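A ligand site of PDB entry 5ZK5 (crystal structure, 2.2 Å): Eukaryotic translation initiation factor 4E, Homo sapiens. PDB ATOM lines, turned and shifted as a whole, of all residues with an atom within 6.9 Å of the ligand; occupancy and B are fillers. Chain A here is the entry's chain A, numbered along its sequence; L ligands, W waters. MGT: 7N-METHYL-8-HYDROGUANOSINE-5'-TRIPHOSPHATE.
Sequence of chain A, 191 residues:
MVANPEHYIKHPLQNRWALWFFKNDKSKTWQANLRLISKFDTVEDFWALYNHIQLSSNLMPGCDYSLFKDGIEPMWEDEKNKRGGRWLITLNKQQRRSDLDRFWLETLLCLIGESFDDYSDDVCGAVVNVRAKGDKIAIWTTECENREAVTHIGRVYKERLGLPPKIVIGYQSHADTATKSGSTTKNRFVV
Merely in contact with the ligand: Met 75 (3.3 Å) and Gln 31 (3.5 Å). Seven residues have an atom within 4 Å of the ligand: Trp 30, Gln 31, Met 75, Trp 76, Glu 77, Arg 131 and Lys 136.
OE1 of Glu 77 is in hydrogen-bond range of N2 of the ligand. NZ of Lys 136 is in salt-bridge range of O2B of the ligand, at 2.7 Å. The guanidinium group of Arg 131 is in salt-bridge range of an oxygen (O1A) of the ligand (2.7 Å). The backbone NH of Trp 76 lies within hydrogen-bond range of an oxygen (O6) of the ligand (2.8 Å). NE1 of Trp 30 sits close to N9 of the ligand, at 3.5 Å.
Water W3 bridges O1A of the ligand (2.7 Å) and NH2 of Arg 131 (3.5 Å).
N of Asn 129 lies within hydrogen-bond range of O of Lys 136 (2.7 Å). OD1 of Asp 64 lies within salt-bridge range of NH1 of Arg 131 (2.9 Å). The guanidinium group (NH1) of Arg 131 lies close to the backbone carbonyl oxygen (O) of Gly 62, 3.5 Å away. The side-chain sulfur of Met 75 is in hydrogen-bond range of the side-chain amide nitrogen of Gln 31.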
ATOM      1  N   PHE A  22      27.524  -1.266   9.329  1.00  0.00           N
ATOM      2  CA  PHE A  22      26.237  -0.768   8.841  1.00  0.00           C
ATOM      3  C   PHE A  22      25.131  -1.502   9.618  1.00  0.00           C
ATOM      4  O   PHE A  22      25.143  -2.712   9.676  1.00  0.00           O
ATOM      5  CB  PHE A  22      26.124  -1.016   7.340  1.00  0.00           C
ATOM      6  CG  PHE A  22      24.824  -0.554   6.734  1.00  0.00           C
ATOM      7  CD1 PHE A  22      23.731  -1.428   6.637  1.00  0.00           C
ATOM      8  CD2 PHE A  22      24.687   0.723   6.225  1.00  0.00           C
ATOM      9  CE1 PHE A  22      22.530  -1.017   6.069  1.00  0.00           C
ATOM     10  CE2 PHE A  22      23.487   1.134   5.657  1.00  0.00           C
ATOM     11  CZ  PHE A  22      22.404   0.269   5.587  1.00  0.00           C
ATOM     12  N   TRP A  30      20.208   5.474   3.630  1.00  0.00           N
ATOM     13  CA  TRP A  30      21.252   4.453   3.595  1.00  0.00           C
ATOM     14  C   TRP A  30      22.581   4.949   4.201  1.00  0.00           C
ATOM     15  O   TRP A  30      23.066   4.327   5.140  1.00  0.00           O
ATOM     16  CB  TRP A  30      21.471   3.908   2.178  1.00  0.00           C
ATOM     17  CG  TRP A  30      22.480   2.813   2.160  1.00  0.00           C
ATOM     18  CD1 TRP A  30      22.263   1.503   2.420  1.00  0.00           C
ATOM     19  CD2 TRP A  30      23.884   2.948   1.917  1.00  0.00           C
ATOM     20  NE1 TRP A  30      23.435   0.793   2.357  1.00  0.00           N
ATOM     21  CE2 TRP A  30      24.447   1.662   2.037  1.00  0.00           C
ATOM     22  CE3 TRP A  30      24.719   4.023   1.596  1.00  0.00           C
ATOM     23  CZ2 TRP A  30      25.815   1.415   1.856  1.00  0.00           C
ATOM     24  CZ3 TRP A  30      26.071   3.790   1.424  1.00  0.00           C
ATOM     25  CH2 TRP A  30      26.609   2.498   1.533  1.00  0.00           C
ATOM     26  N   GLN A  31      23.144   6.055   3.717  1.00  0.00           N
ATOM     27  CA  GLN A  31      24.483   6.468   4.198  1.00  0.00           C
ATOM     28  C   GLN A  31      24.530   7.026   5.626  1.00  0.00           C
ATOM     29  O   GLN A  31      25.618   7.088   6.212  1.00  0.00           O
ATOM     30  CB  GLN A  31      25.268   7.333   3.201  1.00  0.00           C
ATOM     31  CG  GLN A  31      24.641   8.612   2.662  1.00  0.00           C
ATOM     32  CD  GLN A  31      25.078   8.858   1.213  1.00  0.00           C
ATOM     33  OE1 GLN A  31      24.532   8.270   0.279  1.00  0.00           O
ATOM     34  NE2 GLN A  31      26.078   9.709   1.031  1.00  0.00           N
ATOM     35  N   LEU A  34      25.840   4.124   8.197  1.00  0.00           N
ATOM     36  CA  LEU A  34      27.250   3.712   8.191  1.00  0.00           C
ATOM     37  C   LEU A  34      27.972   4.314   9.379  1.00  0.00           C
ATOM     38  O   LEU A  34      27.921   5.530   9.548  1.00  0.00           O
ATOM     39  CB  LEU A  34      27.968   4.228   6.924  1.00  0.00           C
ATOM     40  CG  LEU A  34      27.835   3.484   5.610  1.00  0.00           C
ATOM     41  CD1 LEU A  34      28.470   4.298   4.495  1.00  0.00           C
ATOM     42  CD2 LEU A  34      28.477   2.098   5.696  1.00  0.00           C
ATOM     43  N   GLY A  62      20.473  -7.650   7.816  1.00  0.00           N
ATOM     44  CA  GLY A  62      20.448  -6.228   7.541  1.00  0.00           C
ATOM     45  C   GLY A  62      21.758  -5.504   7.837  1.00  0.00           C
ATOM     46  O   GLY A  62      21.945  -4.372   7.411  1.00  0.00           O
ATOM     47  N   ASP A  64      26.040  -4.912   7.825  1.00  0.00           N
ATOM     48  CA  ASP A  64      27.254  -5.121   7.049  1.00  0.00           C
ATOM     49  C   ASP A  64      28.486  -4.823   7.866  1.00  0.00           C
ATOM     50  O   ASP A  64      28.461  -4.013   8.790  1.00  0.00           O
ATOM     51  CB  ASP A  64      27.358  -4.192   5.817  1.00  0.00           C
ATOM     52  CG  ASP A  64      26.094  -4.105   4.990  1.00  0.00           C
ATOM     53  OD1 ASP A  64      25.311  -5.068   4.918  1.00  0.00           O
ATOM     54  OD2 ASP A  64      25.921  -3.030   4.368  1.00  0.00           O
ATOM     55  N   PRO A  74      32.929   3.267   2.109  1.00  0.00           N
ATOM     56  CA  PRO A  74      32.366   2.103   1.445  1.00  0.00           C
ATOM     57  C   PRO A  74      31.019   2.422   0.775  1.00  0.00           C
ATOM     58  O   PRO A  74      29.989   1.822   1.104  1.00  0.00           O
ATOM     59  CB  PRO A  74      32.210   1.112   2.595  1.00  0.00           C
ATOM     60  CG  PRO A  74      31.887   1.995   3.765  1.00  0.00           C
ATOM     61  CD  PRO A  74      32.657   3.265   3.557  1.00  0.00           C
ATOM     62  N   MET A  75      31.035   3.359  -0.166  1.00  0.00           N
ATOM     63  CA  MET A  75      29.827   3.735  -0.888  1.00  0.00           C
ATOM     64  C   MET A  75      30.147   4.041  -2.338  1.00  0.00           C
ATOM     65  O   MET A  75      31.260   4.519  -2.659  1.00  0.00           O
ATOM     66  CB  MET A  75      29.118   4.906  -0.187  1.00  0.00           C
ATOM     67  CG  MET A  75      29.909   6.204  -0.135  1.00  0.00           C
ATOM     68  SD  MET A  75      29.026   7.577   0.637  1.00  0.00           S
ATOM     69  CE  MET A  75      28.945   7.044   2.337  1.00  0.00           C
ATOM     70  N   TRP A  76      29.185   3.779  -3.224  1.00  0.00           N
ATOM     71  CA  TRP A  76      29.355   4.042  -4.665  1.00  0.00           C
ATOM     72  C   TRP A  76      29.803   5.475  -4.915  1.00  0.00           C
ATOM     73  O   TRP A  76      30.624   5.720  -5.782  1.00  0.00           O
ATOM     74  CB  TRP A  76      28.058   3.817  -5.462  1.00  0.00           C
ATOM     75  CG  TRP A  76      27.406   2.530  -5.227  1.00  0.00           C
ATOM     76  CD1 TRP A  76      28.010   1.308  -5.074  1.00  0.00           C
ATOM     77  CD2 TRP A  76      26.003   2.303  -5.122  1.00  0.00           C
ATOM     78  NE1 TRP A  76      27.058   0.338  -4.877  1.00  0.00           N
ATOM     79  CE2 TRP A  76      25.816   0.923  -4.891  1.00  0.00           C
ATOM     80  CE3 TRP A  76      24.876   3.141  -5.173  1.00  0.00           C
ATOM     81  CZ2 TRP A  76      24.547   0.349  -4.743  1.00  0.00           C
ATOM     82  CZ3 TRP A  76      23.615   2.564  -5.005  1.00  0.00           C
ATOM     83  CH2 TRP A  76      23.467   1.187  -4.793  1.00  0.00           C
ATOM     84  N   GLU A  77      29.262   6.398  -4.124  1.00  0.00           N
ATOM     85  CA  GLU A  77      29.455   7.834  -4.309  1.00  0.00           C
ATOM     86  C   GLU A  77      30.878   8.303  -4.151  1.00  0.00           C
ATOM     87  O   GLU A  77      31.237   9.333  -4.703  1.00  0.00           O
ATOM     88  CB  GLU A  77      28.562   8.626  -3.339  1.00  0.00           C
ATOM     89  CG  GLU A  77      27.081   8.549  -3.661  1.00  0.00           C
ATOM     90  CD  GLU A  77      26.369   7.331  -3.106  1.00  0.00           C
ATOM     91  OE1 GLU A  77      25.127   7.282  -3.242  1.00  0.00           O
ATOM     92  OE2 GLU A  77      26.996   6.403  -2.536  1.00  0.00           O
ATOM     93  N   ARG A  86      32.414  -4.532  -8.388  1.00  0.00           N
ATOM     94  CA  ARG A  86      32.718  -5.531  -7.381  1.00  0.00           C
ATOM     95  C   ARG A  86      32.702  -6.961  -7.872  1.00  0.00           C
ATOM     96  O   ARG A  86      31.867  -7.345  -8.684  1.00  0.00           O
ATOM     97  CB  ARG A  86      31.712  -5.436  -6.235  1.00  0.00           C
ATOM     98  CG  ARG A  86      30.237  -5.460  -6.682  1.00  0.00           C
ATOM     99  CD  ARG A  86      29.302  -5.800  -5.551  1.00  0.00           C
ATOM    100  NE  ARG A  86      27.926  -6.043  -6.007  1.00  0.00           N
ATOM    101  CZ  ARG A  86      26.858  -6.114  -5.200  1.00  0.00           C
ATOM    102  NH1 ARG A  86      25.657  -6.344  -5.711  1.00  0.00           N
ATOM    103  NH2 ARG A  86      26.968  -5.946  -3.873  1.00  0.00           N
ATOM    104  N   VAL A 127      33.106  -5.762   1.224  1.00  0.00           N
ATOM    105  CA  VAL A 127      31.859  -5.698   1.999  1.00  0.00           C
ATOM    106  C   VAL A 127      31.232  -7.082   2.179  1.00  0.00           C
ATOM    107  O   VAL A 127      31.140  -7.850   1.226  1.00  0.00           O
ATOM    108  CB  VAL A 127      30.823  -4.804   1.281  1.00  0.00           C
ATOM    109  CG1 VAL A 127      29.531  -4.709   2.089  1.00  0.00           C
ATOM    110  CG2 VAL A 127      31.407  -3.420   1.036  1.00  0.00           C
ATOM    111  N   ASN A 129      27.533  -8.546   3.393  1.00  0.00           N
ATOM    112  CA  ASN A 129      26.135  -8.245   3.654  1.00  0.00           C
ATOM    113  C   ASN A 129      25.520  -9.486   4.253  1.00  0.00           C
ATOM    114  O   ASN A 129      25.468 -10.541   3.597  1.00  0.00           O
ATOM    115  CB  ASN A 129      25.376  -7.929   2.364  1.00  0.00           C
ATOM    116  CG  ASN A 129      26.007  -6.831   1.562  1.00  0.00           C
ATOM    117  OD1 ASN A 129      26.474  -7.083   0.451  1.00  0.00           O
ATOM    118  ND2 ASN A 129      26.042  -5.610   2.098  1.00  0.00           N
ATOM    119  N   VAL A 130      25.051  -9.369   5.494  1.00  0.00           N
ATOM    120  CA  VAL A 130      24.345 -10.465   6.170  1.00  0.00           C
ATOM    121  C   VAL A 130      22.878 -10.172   5.969  1.00  0.00           C
ATOM    122  O   VAL A 130      22.391  -9.125   6.373  1.00  0.00           O
ATOM    123  CB  VAL A 130      24.685 -10.529   7.677  1.00  0.00           C
ATOM    124  CG1 VAL A 130      23.868 -11.634   8.362  1.00  0.00           C
ATOM    125  CG2 VAL A 130      26.191 -10.776   7.870  1.00  0.00           C
ATOM    126  N   ARG A 131      22.187 -11.071   5.280  1.00  0.00           N
ATOM    127  CA  ARG A 131      20.809 -10.874   4.899  1.00  0.00           C
ATOM    128  C   ARG A 131      20.020 -12.156   5.025  1.00  0.00           C
ATOM    129  O   ARG A 131      20.529 -13.243   4.727  1.00  0.00           O
ATOM    130  CB  ARG A 131      20.733 -10.386   3.460  1.00  0.00           C
ATOM    131  CG  ARG A 131      21.353  -9.024   3.196  1.00  0.00           C
ATOM    132  CD  ARG A 131      20.532  -7.883   3.786  1.00  0.00           C
ATOM    133  NE  ARG A 131      21.125  -6.613   3.396  1.00  0.00           N
ATOM    134  CZ  ARG A 131      22.216  -6.070   3.940  1.00  0.00           C
ATOM    135  NH1 ARG A 131      22.868  -6.650   4.945  1.00  0.00           N
ATOM    136  NH2 ARG A 131      22.665  -4.903   3.469  1.00  0.00           N
ATOM    137  N   LYS A 133      17.636 -13.172   3.131  1.00  0.00           N
ATOM    138  CA  LYS A 133      17.489 -13.823   1.815  1.00  0.00           C
ATOM    139  C   LYS A 133      18.725 -14.551   1.293  1.00  0.00           C
ATOM    140  O   LYS A 133      18.606 -15.366   0.397  1.00  0.00           O
ATOM    141  CB  LYS A 133      17.058 -12.791   0.753  1.00  0.00           C
ATOM    142  N   GLY A 134      19.904 -14.229   1.837  1.00  0.00           N
ATOM    143  CA  GLY A 134      21.177 -14.787   1.330  1.00  0.00           C
ATOM    144  C   GLY A 134      22.306 -13.755   1.434  1.00  0.00           C
ATOM    145  O   GLY A 134      22.143 -12.595   1.043  1.00  0.00           O
ATOM    146  N   LYS A 136      26.125 -11.946   1.099  1.00  0.00           N
ATOM    147  CA  LYS A 136      27.051 -11.601   0.026  1.00  0.00           C
ATOM    148  C   LYS A 136      28.363 -11.086   0.583  1.00  0.00           C
ATOM    149  O   LYS A 136      28.401 -10.401   1.627  1.00  0.00           O
ATOM    150  CB  LYS A 136      26.414 -10.552  -0.886  1.00  0.00           C
ATOM    151  CG  LYS A 136      25.252 -11.071  -1.715  1.00  0.00           C
ATOM    152  CD  LYS A 136      24.446  -9.933  -2.343  1.00  0.00           C
ATOM    153  CE  LYS A 136      23.532  -9.300  -1.318  1.00  0.00           C
ATOM    154  NZ  LYS A 136      22.918  -8.052  -1.829  1.00  0.00           N
ATOM    155  N   TRP A 140      35.507  -4.672  -3.812  1.00  0.00           N
ATOM    156  CA  TRP A 140      35.249  -3.466  -4.558  1.00  0.00           C
ATOM    157  C   TRP A 140      36.579  -2.963  -5.104  1.00  0.00           C
ATOM    158  O   TRP A 140      37.559  -2.859  -4.354  1.00  0.00           O
ATOM    159  CB  TRP A 140      34.654  -2.417  -3.616  1.00  0.00           C
ATOM    160  CG  TRP A 140      33.237  -2.635  -3.231  1.00  0.00           C
ATOM    161  CD1 TRP A 140      32.606  -3.823  -3.011  1.00  0.00           C
ATOM    162  CD2 TRP A 140      32.253  -1.620  -3.011  1.00  0.00           C
ATOM    163  NE1 TRP A 140      31.283  -3.608  -2.649  1.00  0.00           N
ATOM    164  CE2 TRP A 140      31.047  -2.263  -2.647  1.00  0.00           C
ATOM    165  CE3 TRP A 140      32.289  -0.207  -3.044  1.00  0.00           C
ATOM    166  CZ2 TRP A 140      29.882  -1.558  -2.363  1.00  0.00           C
ATOM    167  CZ3 TRP A 140      31.123   0.485  -2.752  1.00  0.00           C
ATOM    168  CH2 TRP A 140      29.935  -0.178  -2.418  1.00  0.00           C
ATOM    169  N   THR A 177      24.736  -1.589 -10.864  1.00  0.00           N
ATOM    170  CA  THR A 177      24.081  -2.012  -9.596  1.00  0.00           C
ATOM    171  C   THR A 177      23.105  -0.941  -9.102  1.00  0.00           C
ATOM    172  O   THR A 177      22.023  -1.271  -8.622  1.00  0.00           O
ATOM    173  CB  THR A 177      25.107  -2.347  -8.472  1.00  0.00           C
ATOM    174  OG1 THR A 177      26.051  -3.318  -8.931  1.00  0.00           O
ATOM    175  CG2 THR A 177      24.398  -2.903  -7.239  1.00  0.00           C
ATOM    176  N   ALA A 178      23.474   0.326  -9.246  1.00  0.00           N
ATOM    177  CA  ALA A 178      22.648   1.456  -8.812  1.00  0.00           C
ATOM    178  C   ALA A 178      21.281   1.543  -9.538  1.00  0.00           C
ATOM    179  O   ALA A 178      20.259   1.814  -8.907  1.00  0.00           O
ATOM    180  CB  ALA A 178      23.405   2.771  -8.978  1.00  0.00           C
HETATM  181  PG  MGT L   1      19.311  -5.837  -2.806  1.00  0.00           P
HETATM  182  O1G MGT L   1      20.654  -5.504  -3.430  1.00  0.00           O
HETATM  183  O2G MGT L   1      19.015  -7.332  -2.774  1.00  0.00           O
HETATM  184  O3G MGT L   1      18.188  -5.015  -3.378  1.00  0.00           O
HETATM  185  O3B MGT L   1      19.361  -5.389  -1.235  1.00  0.00           O
HETATM  186  PB  MGT L   1      20.553  -5.781  -0.231  1.00  0.00           P
HETATM  187  O1B MGT L   1      20.276  -5.244   1.159  1.00  0.00           O
HETATM  188  O2B MGT L   1      20.834  -7.243  -0.369  1.00  0.00           O
HETATM  189  O3A MGT L   1      21.824  -5.021  -0.890  1.00  0.00           O
HETATM  190  PA  MGT L   1      22.527  -3.658  -0.372  1.00  0.00           P
HETATM  191  O1A MGT L   1      22.431  -3.509   1.129  1.00  0.00           O
HETATM  192  O2A MGT L   1      23.864  -3.489  -1.050  1.00  0.00           O
HETATM  193  O5' MGT L   1      21.624  -2.521  -1.029  1.00  0.00           O
HETATM  194  C5' MGT L   1      20.253  -2.350  -0.772  1.00  0.00           C
HETATM  195  C4' MGT L   1      19.945  -0.876  -0.924  1.00  0.00           C
HETATM  196  O4' MGT L   1      20.772  -0.065  -0.071  1.00  0.00           O
HETATM  197  C3' MGT L   1      20.195  -0.415  -2.359  1.00  0.00           C
HETATM  198  O3' MGT L   1      19.086  -0.665  -3.217  1.00  0.00           O
HETATM  199  C2' MGT L   1      20.530   1.058  -2.180  1.00  0.00           C
HETATM  200  O2' MGT L   1      19.384   1.885  -2.235  1.00  0.00           O
HETATM  201  C1' MGT L   1      21.142   1.125  -0.790  1.00  0.00           C
HETATM  202  N9  MGT L   1      22.604   1.269  -1.006  1.00  0.00           N
HETATM  203  C8  MGT L   1      23.428   0.047  -0.912  1.00  0.00           C
HETATM  204  N7  MGT L   1      24.713   0.676  -1.194  1.00  0.00           N
HETATM  205  CM7 MGT L   1      25.827  -0.291  -1.184  1.00  0.00           C
HETATM  206  C5  MGT L   1      24.657   1.984  -1.437  1.00  0.00           C
HETATM  207  C6  MGT L   1      25.653   3.009  -1.779  1.00  0.00           C
HETATM  208  O6  MGT L   1      26.871   2.779  -1.910  1.00  0.00           O
HETATM  209  N1  MGT L   1      25.191   4.242  -1.938  1.00  0.00           N
HETATM  210  C2  MGT L   1      23.880   4.550  -1.819  1.00  0.00           C
HETATM  211  N2  MGT L   1      23.471   5.813  -1.995  1.00  0.00           N
HETATM  212  N3  MGT L   1      22.897   3.652  -1.515  1.00  0.00           N
HETATM  213  C4  MGT L   1      23.244   2.379  -1.316  1.00  0.00           C
HETATM  214  O   HOH W   1      24.264  -3.053  -3.556  1.00  0.00           O
HETATM  215  O   HOH W   2      19.285  -9.104   0.161  1.00  0.00           O
HETATM  216  O   HOH W   3      20.656  -2.198   2.710  1.00  0.00           O
